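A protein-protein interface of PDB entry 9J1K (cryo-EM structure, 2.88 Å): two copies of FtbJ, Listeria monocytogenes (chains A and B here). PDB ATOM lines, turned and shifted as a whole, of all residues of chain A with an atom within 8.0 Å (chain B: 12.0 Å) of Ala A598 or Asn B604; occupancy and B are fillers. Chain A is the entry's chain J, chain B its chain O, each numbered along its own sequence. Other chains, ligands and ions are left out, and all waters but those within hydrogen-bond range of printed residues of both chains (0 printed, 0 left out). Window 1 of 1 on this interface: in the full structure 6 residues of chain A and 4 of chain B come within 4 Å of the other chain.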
ATOM      1  N   ASP A 593      19.643  12.492 -21.554  1.00  0.00           N
ATOM      2  CA  ASP A 593      20.690  12.306 -20.561  1.00  0.00           C
ATOM      3  C   ASP A 593      21.583  11.137 -20.957  1.00  0.00           C
ATOM      4  O   ASP A 593      21.143  10.190 -21.615  1.00  0.00           O
ATOM      5  CB  ASP A 593      20.057  12.084 -19.181  1.00  0.00           C
ATOM      6  CG  ASP A 593      21.076  11.812 -18.075  1.00  0.00           C
ATOM      7  OD1 ASP A 593      20.905  12.393 -16.983  1.00  0.00           O
ATOM      8  OD2 ASP A 593      22.016  11.012 -18.256  1.00  0.00           O
ATOM      9  N   ASP A 594      22.849  11.209 -20.549  1.00  0.00           N
ATOM     10  CA  ASP A 594      23.820  10.171 -20.870  1.00  0.00           C
ATOM     11  C   ASP A 594      24.142   9.262 -19.691  1.00  0.00           C
ATOM     12  O   ASP A 594      24.491   8.095 -19.900  1.00  0.00           O
ATOM     13  CB  ASP A 594      25.107  10.809 -21.405  1.00  0.00           C
ATOM     14  CG  ASP A 594      25.770  11.744 -20.402  1.00  0.00           C
ATOM     15  OD1 ASP A 594      25.385  11.751 -19.214  1.00  0.00           O
ATOM     16  OD2 ASP A 594      26.691  12.480 -20.812  1.00  0.00           O
ATOM     17  N   LYS A 595      24.041   9.769 -18.460  1.00  0.00           N
ATOM     18  CA  LYS A 595      24.385   8.962 -17.293  1.00  0.00           C
ATOM     19  C   LYS A 595      23.433   7.781 -17.136  1.00  0.00           C
ATOM     20  O   LYS A 595      23.866   6.650 -16.884  1.00  0.00           O
ATOM     21  CB  LYS A 595      24.376   9.834 -16.039  1.00  0.00           C
ATOM     22  CG  LYS A 595      25.654  10.635 -15.834  1.00  0.00           C
ATOM     23  CD  LYS A 595      25.637  11.499 -14.569  1.00  0.00           C
ATOM     24  CE  LYS A 595      25.811  10.719 -13.258  1.00  0.00           C
ATOM     25  NZ  LYS A 595      24.914   9.549 -13.042  1.00  0.00           N
ATOM     26  N   VAL A 596      22.130   8.025 -17.287  1.00  0.00           N
ATOM     27  CA  VAL A 596      21.158   6.945 -17.155  1.00  0.00           C
ATOM     28  C   VAL A 596      21.314   5.944 -18.293  1.00  0.00           C
ATOM     29  O   VAL A 596      21.176   4.731 -18.093  1.00  0.00           O
ATOM     30  CB  VAL A 596      19.730   7.516 -17.094  1.00  0.00           C
ATOM     31  CG1 VAL A 596      19.445   8.072 -15.711  1.00  0.00           C
ATOM     32  CG2 VAL A 596      19.544   8.590 -18.150  1.00  0.00           C
ATOM     33  N   VAL A 597      21.601   6.434 -19.500  1.00  0.00           N
ATOM     34  CA  VAL A 597      21.832   5.539 -20.629  1.00  0.00           C
ATOM     35  C   VAL A 597      23.028   4.642 -20.351  1.00  0.00           C
ATOM     36  O   VAL A 597      22.979   3.426 -20.575  1.00  0.00           O
ATOM     37  CB  VAL A 597      22.019   6.350 -21.924  1.00  0.00           C
ATOM     38  CG1 VAL A 597      22.663   5.493 -23.001  1.00  0.00           C
ATOM     39  CG2 VAL A 597      20.686   6.898 -22.400  1.00  0.00           C
ATOM     40  N   ALA A 598      24.115   5.224 -19.842  1.00  0.00           N
ATOM     41  CA  ALA A 598      25.296   4.433 -19.519  1.00  0.00           C
ATOM     42  C   ALA A 598      24.997   3.412 -18.430  1.00  0.00           C
ATOM     43  O   ALA A 598      25.458   2.268 -18.502  1.00  0.00           O
ATOM     44  CB  ALA A 598      26.441   5.348 -19.094  1.00  0.00           C
ATOM     45  N   GLU A 599      24.234   3.806 -17.409  1.00  0.00           N
ATOM     46  CA  GLU A 599      23.952   2.886 -16.310  1.00  0.00           C
ATOM     47  C   GLU A 599      23.083   1.724 -16.783  1.00  0.00           C
ATOM     48  O   GLU A 599      23.320   0.569 -16.408  1.00  0.00           O
ATOM     49  CB  GLU A 599      23.344   3.674 -15.135  1.00  0.00           C
ATOM     50  CG  GLU A 599      22.722   2.931 -13.921  1.00  0.00           C
ATOM     51  CD  GLU A 599      21.426   2.164 -14.166  1.00  0.00           C
ATOM     52  OE1 GLU A 599      20.888   2.175 -15.289  1.00  0.00           O
ATOM     53  OE2 GLU A 599      20.934   1.542 -13.204  1.00  0.00           O
ATOM     54  N   VAL A 600      22.087   2.002 -17.626  1.00  0.00           N
ATOM     55  CA  VAL A 600      21.245   0.932 -18.157  1.00  0.00           C
ATOM     56  C   VAL A 600      22.047   0.017 -19.075  1.00  0.00           C
ATOM     57  O   VAL A 600      21.888  -1.212 -19.045  1.00  0.00           O
ATOM     58  CB  VAL A 600      20.016   1.522 -18.869  1.00  0.00           C
ATOM     59  CG1 VAL A 600      19.361   0.476 -19.755  1.00  0.00           C
ATOM     60  CG2 VAL A 600      19.026   2.049 -17.846  1.00  0.00           C
ATOM     61  N   VAL A 601      22.912   0.596 -19.912  1.00  0.00           N
ATOM     62  CA  VAL A 601      23.766  -0.215 -20.774  1.00  0.00           C
ATOM     63  C   VAL A 601      24.655  -1.117 -19.933  1.00  0.00           C
ATOM     64  O   VAL A 601      24.833  -2.302 -20.241  1.00  0.00           O
ATOM     65  CB  VAL A 601      24.590   0.688 -21.710  1.00  0.00           C
ATOM     66  CG1 VAL A 601      25.750  -0.083 -22.314  1.00  0.00           C
ATOM     67  CG2 VAL A 601      23.707   1.260 -22.806  1.00  0.00           C
ATOM     68  N   SER A 602      25.219  -0.575 -18.852  1.00  0.00           N
ATOM     69  CA  SER A 602      26.058  -1.374 -17.968  1.00  0.00           C
ATOM     70  C   SER A 602      25.263  -2.501 -17.324  1.00  0.00           C
ATOM     71  O   SER A 602      25.763  -3.623 -17.196  1.00  0.00           O
ATOM     72  CB  SER A 602      26.687  -0.481 -16.901  1.00  0.00           C
ATOM     73  OG  SER A 602      27.505   0.517 -17.487  1.00  0.00           O
ATOM     74  N   ARG A 603      24.025  -2.224 -16.908  1.00  0.00           N
ATOM     75  CA  ARG A 603      23.209  -3.270 -16.295  1.00  0.00           C
ATOM     76  C   ARG A 603      22.894  -4.384 -17.287  1.00  0.00           C
ATOM     77  O   ARG A 603      22.963  -5.571 -16.945  1.00  0.00           O
ATOM     78  CB  ARG A 603      21.922  -2.673 -15.729  1.00  0.00           C
ATOM     79  CG  ARG A 603      21.973  -2.436 -14.230  1.00  0.00           C
ATOM     80  CD  ARG A 603      20.587  -2.230 -13.643  1.00  0.00           C
ATOM     81  NE  ARG A 603      20.054  -0.904 -13.925  1.00  0.00           N
ATOM     82  CZ  ARG A 603      19.001  -0.668 -14.694  1.00  0.00           C
ATOM     83  NH1 ARG A 603      18.350  -1.650 -15.294  1.00  0.00           N
ATOM     84  NH2 ARG A 603      18.589   0.585 -14.865  1.00  0.00           N
ATOM     85  N   ASN A 604      22.543  -4.024 -18.523  1.00  0.00           N
ATOM     86  CA  ASN A 604      22.253  -5.044 -19.528  1.00  0.00           C
ATOM     87  C   ASN A 604      23.500  -5.852 -19.873  1.00  0.00           C
ATOM     88  O   ASN A 604      23.431  -7.078 -20.047  1.00  0.00           O
ATOM     89  CB  ASN A 604      21.664  -4.394 -20.776  1.00  0.00           C
ATOM     90  CG  ASN A 604      20.224  -3.967 -20.580  1.00  0.00           C
ATOM     91  OD1 ASN A 604      19.296  -4.667 -20.986  1.00  0.00           O
ATOM     92  ND2 ASN A 604      20.029  -2.820 -19.943  1.00  0.00           N
ATOM     93  N   GLN A 605      24.650  -5.184 -19.969  1.00  0.00           N
ATOM     94  CA  GLN A 605      25.897  -5.900 -20.205  1.00  0.00           C
ATOM     95  C   GLN A 605      26.213  -6.840 -19.052  1.00  0.00           C
ATOM     96  O   GLN A 605      26.725  -7.944 -19.265  1.00  0.00           O
ATOM     97  CB  GLN A 605      27.037  -4.907 -20.425  1.00  0.00           C
ATOM     98  CG  GLN A 605      26.922  -4.102 -21.706  1.00  0.00           C
ATOM     99  CD  GLN A 605      28.247  -3.527 -22.155  1.00  0.00           C
ATOM    100  OE1 GLN A 605      28.782  -3.913 -23.194  1.00  0.00           O
ATOM    101  NE2 GLN A 605      28.781  -2.590 -21.381  1.00  0.00           N
ATOM    102  N   MET B 592      20.319   7.546 -35.867  1.00  0.00           N
ATOM    103  CA  MET B 592      21.208   8.165 -34.896  1.00  0.00           C
ATOM    104  C   MET B 592      22.505   7.377 -34.830  1.00  0.00           C
ATOM    105  O   MET B 592      22.496   6.140 -34.845  1.00  0.00           O
ATOM    106  CB  MET B 592      20.548   8.262 -33.513  1.00  0.00           C
ATOM    107  CG  MET B 592      19.877   7.000 -33.025  1.00  0.00           C
ATOM    108  SD  MET B 592      20.937   6.119 -31.875  1.00  0.00           S
ATOM    109  CE  MET B 592      20.250   6.646 -30.306  1.00  0.00           C
ATOM    110  N   ASP B 594      25.846   5.466 -33.918  1.00  0.00           N
ATOM    111  CA  ASP B 594      26.145   4.491 -32.880  1.00  0.00           C
ATOM    112  C   ASP B 594      27.547   4.627 -32.302  1.00  0.00           C
ATOM    113  O   ASP B 594      27.743   4.344 -31.117  1.00  0.00           O
ATOM    114  CB  ASP B 594      25.956   3.070 -33.427  1.00  0.00           C
ATOM    115  CG  ASP B 594      26.782   2.803 -34.675  1.00  0.00           C
ATOM    116  OD1 ASP B 594      27.766   3.530 -34.927  1.00  0.00           O
ATOM    117  OD2 ASP B 594      26.439   1.859 -35.414  1.00  0.00           O
ATOM    118  N   LYS B 595      28.524   5.041 -33.112  1.00  0.00           N
ATOM    119  CA  LYS B 595      29.885   5.202 -32.611  1.00  0.00           C
ATOM    120  C   LYS B 595      29.956   6.285 -31.542  1.00  0.00           C
ATOM    121  O   LYS B 595      30.635   6.117 -30.521  1.00  0.00           O
ATOM    122  CB  LYS B 595      30.830   5.526 -33.766  1.00  0.00           C
ATOM    123  CG  LYS B 595      31.116   4.343 -34.680  1.00  0.00           C
ATOM    124  CD  LYS B 595      32.014   4.679 -35.880  1.00  0.00           C
ATOM    125  CE  LYS B 595      33.474   5.021 -35.535  1.00  0.00           C
ATOM    126  NZ  LYS B 595      33.724   6.054 -34.491  1.00  0.00           N
ATOM    127  N   VAL B 596      29.264   7.404 -31.760  1.00  0.00           N
ATOM    128  CA  VAL B 596      29.267   8.489 -30.781  1.00  0.00           C
ATOM    129  C   VAL B 596      28.616   8.036 -29.481  1.00  0.00           C
ATOM    130  O   VAL B 596      29.109   8.331 -28.384  1.00  0.00           O
ATOM    131  CB  VAL B 596      28.570   9.730 -31.364  1.00  0.00           C
ATOM    132  CG1 VAL B 596      28.366  10.784 -30.288  1.00  0.00           C
ATOM    133  CG2 VAL B 596      29.376  10.291 -32.523  1.00  0.00           C
ATOM    134  N   VAL B 597      27.496   7.317 -29.583  1.00  0.00           N
ATOM    135  CA  VAL B 597      26.823   6.812 -28.390  1.00  0.00           C
ATOM    136  C   VAL B 597      27.728   5.849 -27.639  1.00  0.00           C
ATOM    137  O   VAL B 597      27.826   5.896 -26.406  1.00  0.00           O
ATOM    138  CB  VAL B 597      25.486   6.150 -28.773  1.00  0.00           C
ATOM    139  CG1 VAL B 597      24.891   5.422 -27.582  1.00  0.00           C
ATOM    140  CG2 VAL B 597      24.517   7.190 -29.302  1.00  0.00           C
ATOM    141  N   ALA B 598      28.408   4.962 -28.368  1.00  0.00           N
ATOM    142  CA  ALA B 598      29.318   4.021 -27.728  1.00  0.00           C
ATOM    143  C   ALA B 598      30.461   4.745 -27.029  1.00  0.00           C
ATOM    144  O   ALA B 598      30.845   4.379 -25.914  1.00  0.00           O
ATOM    145  CB  ALA B 598      29.859   3.033 -28.758  1.00  0.00           C
ATOM    146  N   GLU B 599      31.018   5.777 -27.666  1.00  0.00           N
ATOM    147  CA  GLU B 599      32.123   6.510 -27.054  1.00  0.00           C
ATOM    148  C   GLU B 599      31.660   7.248 -25.803  1.00  0.00           C
ATOM    149  O   GLU B 599      32.372   7.278 -24.791  1.00  0.00           O
ATOM    150  CB  GLU B 599      32.762   7.433 -28.111  1.00  0.00           C
ATOM    151  CG  GLU B 599      33.817   8.498 -27.692  1.00  0.00           C
ATOM    152  CD  GLU B 599      33.328   9.633 -26.797  1.00  0.00           C
ATOM    153  OE1 GLU B 599      34.177  10.446 -26.375  1.00  0.00           O
ATOM    154  OE2 GLU B 599      32.109   9.794 -26.606  1.00  0.00           O
ATOM    155  N   VAL B 600      30.466   7.846 -25.847  1.00  0.00           N
ATOM    156  CA  VAL B 600      29.937   8.533 -24.670  1.00  0.00           C
ATOM    157  C   VAL B 600      29.704   7.544 -23.535  1.00  0.00           C
ATOM    158  O   VAL B 600      30.037   7.816 -22.372  1.00  0.00           O
ATOM    159  CB  VAL B 600      28.650   9.298 -25.030  1.00  0.00           C
ATOM    160  CG1 VAL B 600      27.792   9.515 -23.792  1.00  0.00           C
ATOM    161  CG2 VAL B 600      28.988  10.623 -25.690  1.00  0.00           C
ATOM    162  N   VAL B 601      29.130   6.381 -23.853  1.00  0.00           N
ATOM    163  CA  VAL B 601      28.884   5.367 -22.833  1.00  0.00           C
ATOM    164  C   VAL B 601      30.199   4.890 -22.235  1.00  0.00           C
ATOM    165  O   VAL B 601      30.309   4.693 -21.019  1.00  0.00           O
ATOM    166  CB  VAL B 601      28.070   4.200 -23.423  1.00  0.00           C
ATOM    167  CG1 VAL B 601      28.104   2.997 -22.495  1.00  0.00           C
ATOM    168  CG2 VAL B 601      26.638   4.633 -23.681  1.00  0.00           C
ATOM    169  N   SER B 602      31.216   4.698 -23.077  1.00  0.00           N
ATOM    170  CA  SER B 602      32.519   4.272 -22.580  1.00  0.00           C
ATOM    171  C   SER B 602      33.129   5.318 -21.658  1.00  0.00           C
ATOM    172  O   SER B 602      33.711   4.977 -20.624  1.00  0.00           O
ATOM    173  CB  SER B 602      33.454   3.980 -23.754  1.00  0.00           C
ATOM    174  OG  SER B 602      32.922   2.965 -24.587  1.00  0.00           O
ATOM    175  N   ARG B 603      33.005   6.598 -22.015  1.00  0.00           N
ATOM    176  CA  ARG B 603      33.536   7.652 -21.154  1.00  0.00           C
ATOM    177  C   ARG B 603      32.818   7.686 -19.809  1.00  0.00           C
ATOM    178  O   ARG B 603      33.455   7.837 -18.758  1.00  0.00           O
ATOM    179  CB  ARG B 603      33.434   9.005 -21.855  1.00  0.00           C
ATOM    180  CG  ARG B 603      34.745   9.483 -22.454  1.00  0.00           C
ATOM    181  CD  ARG B 603      34.735  10.982 -22.693  1.00  0.00           C
ATOM    182  NE  ARG B 603      34.000  11.338 -23.900  1.00  0.00           N
ATOM    183  CZ  ARG B 603      32.861  12.014 -23.911  1.00  0.00           C
ATOM    184  NH1 ARG B 603      32.290  12.424 -22.790  1.00  0.00           N
ATOM    185  NH2 ARG B 603      32.278  12.287 -25.075  1.00  0.00           N
ATOM    186  N   ASN B 604      31.491   7.547 -19.820  1.00  0.00           N
ATOM    187  CA  ASN B 604      30.748   7.545 -18.562  1.00  0.00           C
ATOM    188  C   ASN B 604      31.102   6.331 -17.708  1.00  0.00           C
ATOM    189  O   ASN B 604      31.226   6.439 -16.480  1.00  0.00           O
ATOM    190  CB  ASN B 604      29.249   7.593 -18.841  1.00  0.00           C
ATOM    191  CG  ASN B 604      28.755   8.997 -19.118  1.00  0.00           C
ATOM    192  OD1 ASN B 604      28.221   9.665 -18.233  1.00  0.00           O
ATOM    193  ND2 ASN B 604      28.937   9.455 -20.350  1.00  0.00           N
ATOM    194  N   GLN B 605      31.269   5.167 -18.339  1.00  0.00           N
ATOM    195  CA  GLN B 605      31.680   3.978 -17.601  1.00  0.00           C
ATOM    196  C   GLN B 605      33.075   4.151 -17.020  1.00  0.00           C
ATOM    197  O   GLN B 605      33.355   3.687 -15.911  1.00  0.00           O
ATOM    198  CB  GLN B 605      31.619   2.748 -18.504  1.00  0.00           C
ATOM    199  CG  GLN B 605      30.214   2.367 -18.935  1.00  0.00           C
ATOM    200  CD  GLN B 605      30.117   0.932 -19.404  1.00  0.00           C
ATOM    201  OE1 GLN B 605      29.442   0.109 -18.788  1.00  0.00           O
ATOM    202  NE2 GLN B 605      30.796   0.622 -20.501  1.00  0.00           N
ATOM    203  N   ALA B 606      33.968   4.812 -17.759  1.00  0.00           N
ATOM    204  CA  ALA B 606      35.293   5.109 -17.227  1.00  0.00           C
ATOM    205  C   ALA B 606      35.205   6.030 -16.020  1.00  0.00           C
ATOM    206  O   ALA B 606      35.937   5.853 -15.040  1.00  0.00           O
ATOM    207  CB  ALA B 606      36.169   5.733 -18.310  1.00  0.00           C
ATOM    208  N   ASN B 607      34.324   7.029 -16.079  1.00  0.00           N
ATOM    209  CA  ASN B 607      34.135   7.916 -14.935  1.00  0.00           C
ATOM    210  C   ASN B 607      33.656   7.138 -13.714  1.00  0.00           C
ATOM    211  O   ASN B 607      34.170   7.317 -12.602  1.00  0.00           O
ATOM    212  CB  ASN B 607      33.143   9.023 -15.289  1.00  0.00           C
ATOM    213  CG  ASN B 607      33.766  10.116 -16.131  1.00  0.00           C
ATOM    214  OD1 ASN B 607      34.970  10.107 -16.387  1.00  0.00           O
ATOM    215  ND2 ASN B 607      32.949  11.066 -16.566  1.00  0.00           N
ATOM    216  N   SER B 608      32.671   6.258 -13.911  1.00  0.00           N
ATOM    217  CA  SER B 608      32.168   5.454 -12.799  1.00  0.00           C
ATOM    218  C   SER B 608      33.249   4.528 -12.250  1.00  0.00           C
ATOM    219  O   SER B 608      33.370   4.353 -11.031  1.00  0.00           O
ATOM    220  CB  SER B 608      30.949   4.648 -13.246  1.00  0.00           C
ATOM    221  OG  SER B 608      29.886   5.504 -13.624  1.00  0.00           O
ATOM    222  N   PHE B 609      34.038   3.920 -13.138  1.00  0.00           N
ATOM    223  CA  PHE B 609      35.111   3.034 -12.704  1.00  0.00           C
ATOM    224  C   PHE B 609      36.160   3.793 -11.905  1.00  0.00           C
ATOM    225  O   PHE B 609      36.664   3.290 -10.895  1.00  0.00           O
ATOM    226  CB  PHE B 609      35.743   2.353 -13.918  1.00  0.00           C
ATOM    227  CG  PHE B 609      36.886   1.443 -13.579  1.00  0.00           C
ATOM    228  CD1 PHE B 609      36.655   0.127 -13.225  1.00  0.00           C
ATOM    229  CD2 PHE B 609      38.192   1.899 -13.626  1.00  0.00           C
ATOM    230  CE1 PHE B 609      37.703  -0.715 -12.916  1.00  0.00           C
ATOM    231  CE2 PHE B 609      39.242   1.061 -13.317  1.00  0.00           C
ATOM    232  CZ  PHE B 609      38.998  -0.247 -12.963  1.00  0.00           C
ATOM    233  N   ASP B 610      36.511   5.000 -12.350  1.00  0.00           N
ATOM    234  CA  ASP B 610      37.463   5.816 -11.603  1.00  0.00           C
ATOM    235  C   ASP B 610      36.909   6.188 -10.236  1.00  0.00           C
ATOM    236  O   ASP B 610      37.643   6.186  -9.240  1.00  0.00           O
ATOM    237  CB  ASP B 610      37.816   7.071 -12.400  1.00  0.00           C
ATOM    238  CG  ASP B 610      38.848   6.806 -13.476  1.00  0.00           C
ATOM    239  OD1 ASP B 610      39.510   5.749 -13.418  1.00  0.00           O
ATOM    240  OD2 ASP B 610      38.996   7.654 -14.380  1.00  0.00           O
ATOM    241  N   GLN B 611      35.618   6.516 -10.169  1.00  0.00           N
ATOM    242  CA  GLN B 611      34.992   6.806  -8.884  1.00  0.00           C
ATOM    243  C   GLN B 611      35.090   5.610  -7.944  1.00  0.00           C
ATOM    244  O   GLN B 611      35.483   5.748  -6.777  1.00  0.00           O
ATOM    245  CB  GLN B 611      33.533   7.202  -9.099  1.00  0.00           C
ATOM    246  CG  GLN B 611      32.943   8.049  -7.993  1.00  0.00           C
ATOM    247  CD  GLN B 611      31.730   8.830  -8.451  1.00  0.00           C
ATOM    248  OE1 GLN B 611      31.323   8.743  -9.610  1.00  0.00           O
ATOM    249  NE2 GLN B 611      31.141   9.598  -7.543  1.00  0.00           N
ATOM    250  N   TYR B 612      34.743   4.422  -8.442  1.00  0.00           N
ATOM    251  CA  TYR B 612      34.793   3.226  -7.608  1.00  0.00           C
ATOM    252  C   TYR B 612      36.219   2.912  -7.172  1.00  0.00           C
ATOM    253  O   TYR B 612      36.450   2.499  -6.030  1.00  0.00           O
ATOM    254  CB  TYR B 612      34.180   2.039  -8.349  1.00  0.00           C
ATOM    255  CG  TYR B 612      32.672   2.014  -8.297  1.00  0.00           C
ATOM    256  CD1 TYR B 612      32.002   1.970  -7.082  1.00  0.00           C
ATOM    257  CD2 TYR B 612      31.916   2.040  -9.459  1.00  0.00           C
ATOM    258  CE1 TYR B 612      30.624   1.950  -7.026  1.00  0.00           C
ATOM    259  CE2 TYR B 612      30.536   2.021  -9.413  1.00  0.00           C
ATOM    260  CZ  TYR B 612      29.896   1.975  -8.195  1.00  0.00           C
ATOM    261  OH  TYR B 612      28.522   1.955  -8.146  1.00  0.00           O
ATOM    262  N   ASN B 613      37.187   3.092  -8.072  1.00  0.00           N
ATOM    263  CA  ASN B 613      38.584   2.866  -7.715  1.00  0.00           C
ATOM    264  C   ASN B 613      39.036   3.833  -6.629  1.00  0.00           C
ATOM    265  O   ASN B 613      39.726   3.437  -5.683  1.00  0.00           O
ATOM    266  CB  ASN B 613      39.466   2.995  -8.957  1.00  0.00           C
ATOM    267  CG  ASN B 613      40.945   3.049  -8.625  1.00  0.00           C
ATOM    268  OD1 ASN B 613      41.407   2.422  -7.673  1.00  0.00           O
ATOM    269  ND2 ASN B 613      41.697   3.803  -9.417  1.00  0.00           N
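The side-chain hydroxyl (OG) of Ser A602 sits close to the side-chain amide oxygen (OE1) of Gln B605 (2.4 Å).
The backbone carbonyl oxygen of Asn B604 lies within hydrogen-bond range of the side-chain hydroxyl of Ser B608 (3.3 Å).
The side-chain hydroxyl of Ser A602 sits at hydrogen-bond distance from the backbone carbonyl oxygen of Ala A598, at 2.9 Å.
The side-chain amide nitrogen (ND2) of Asn B604 is in hydrogen-bond range of the backbone carbonyl oxygen (O) of Val B600 (2.8 Å).
Among the printed residues, pairs that only touch across the chains: Ala A598 with Asn B604 (3.6 Å), Lys A595 with Asn B604 (3.6 Å), Asp A594 with Asn B604 (3.7 Å), Gln A605 with Gln B605 (3.8 Å), Asp A594 with Val B600 (3.8 Å) and Val A601 with Val B601 (3.9 Å).
Asp A594 touches two residues of chain B.
Lys A595 touches one residue of chain B.
Val A596 touches none of the printed residues of chain B.
No residue of chain B comes within 4 Å of Val A597.
Ala A598 touches just one residue of chain B: Asn B604 (3.6 Å).
No residue of chain B comes within 4 Å of Glu A599.
Val A600 touches none of the printed residues of chain B.
Ser A602 touches just one residue of chain B: Gln B605 (2.4 Å).
Of the printed residues of chain B, Gln A605 touches Gln B605 (3.8 Å).
Glu B599 touches none of the printed residues of chain A.
Printed residues of chain A within 4 Å of Val B600: Asp A594 (3.8 Å).
Of the printed residues of chain A, Val B601 touches Val A601.
Asn B604 touches just these residues of chain A: Asp A594, Lys A595 and Ala A598.
Of the printed residues of chain A, Gln B605 touches Ser A602 and Gln A605.
Of the 21 printed residues of chain B, 4 touch a printed residue of chain A.
Of the 13 printed residues of chain A, 6 touch a printed residue of chain B.
Printed residues of chain A that touch a printed residue of chain B: Asp A594, Lys A595, Ala A598, Val A601, Ser A602 and Gln A605.
Hydrophobic or aromatic side chains of chain A within 4 Å of the printed part of chain B: Ala A598 and Val A601.
Asp A594 touches Asn B604, but with the chains exchanged Asn A604 does not touch Asp B594 (14.8 Å).
Lys A595 touches Asn B604, but with the chains exchanged Asn A604 does not touch Lys B595 (16.9 Å).
Ser A602 touches Gln B605, but with the chains exchanged Gln A605 does not touch Ser B602 (7.6 Å).
Gln B605 touches its own counterpart, Gln A605.
Of the 7 pairs that touch across the chains among the printed residues, 2 have their exchanged pair printed and touching as well.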
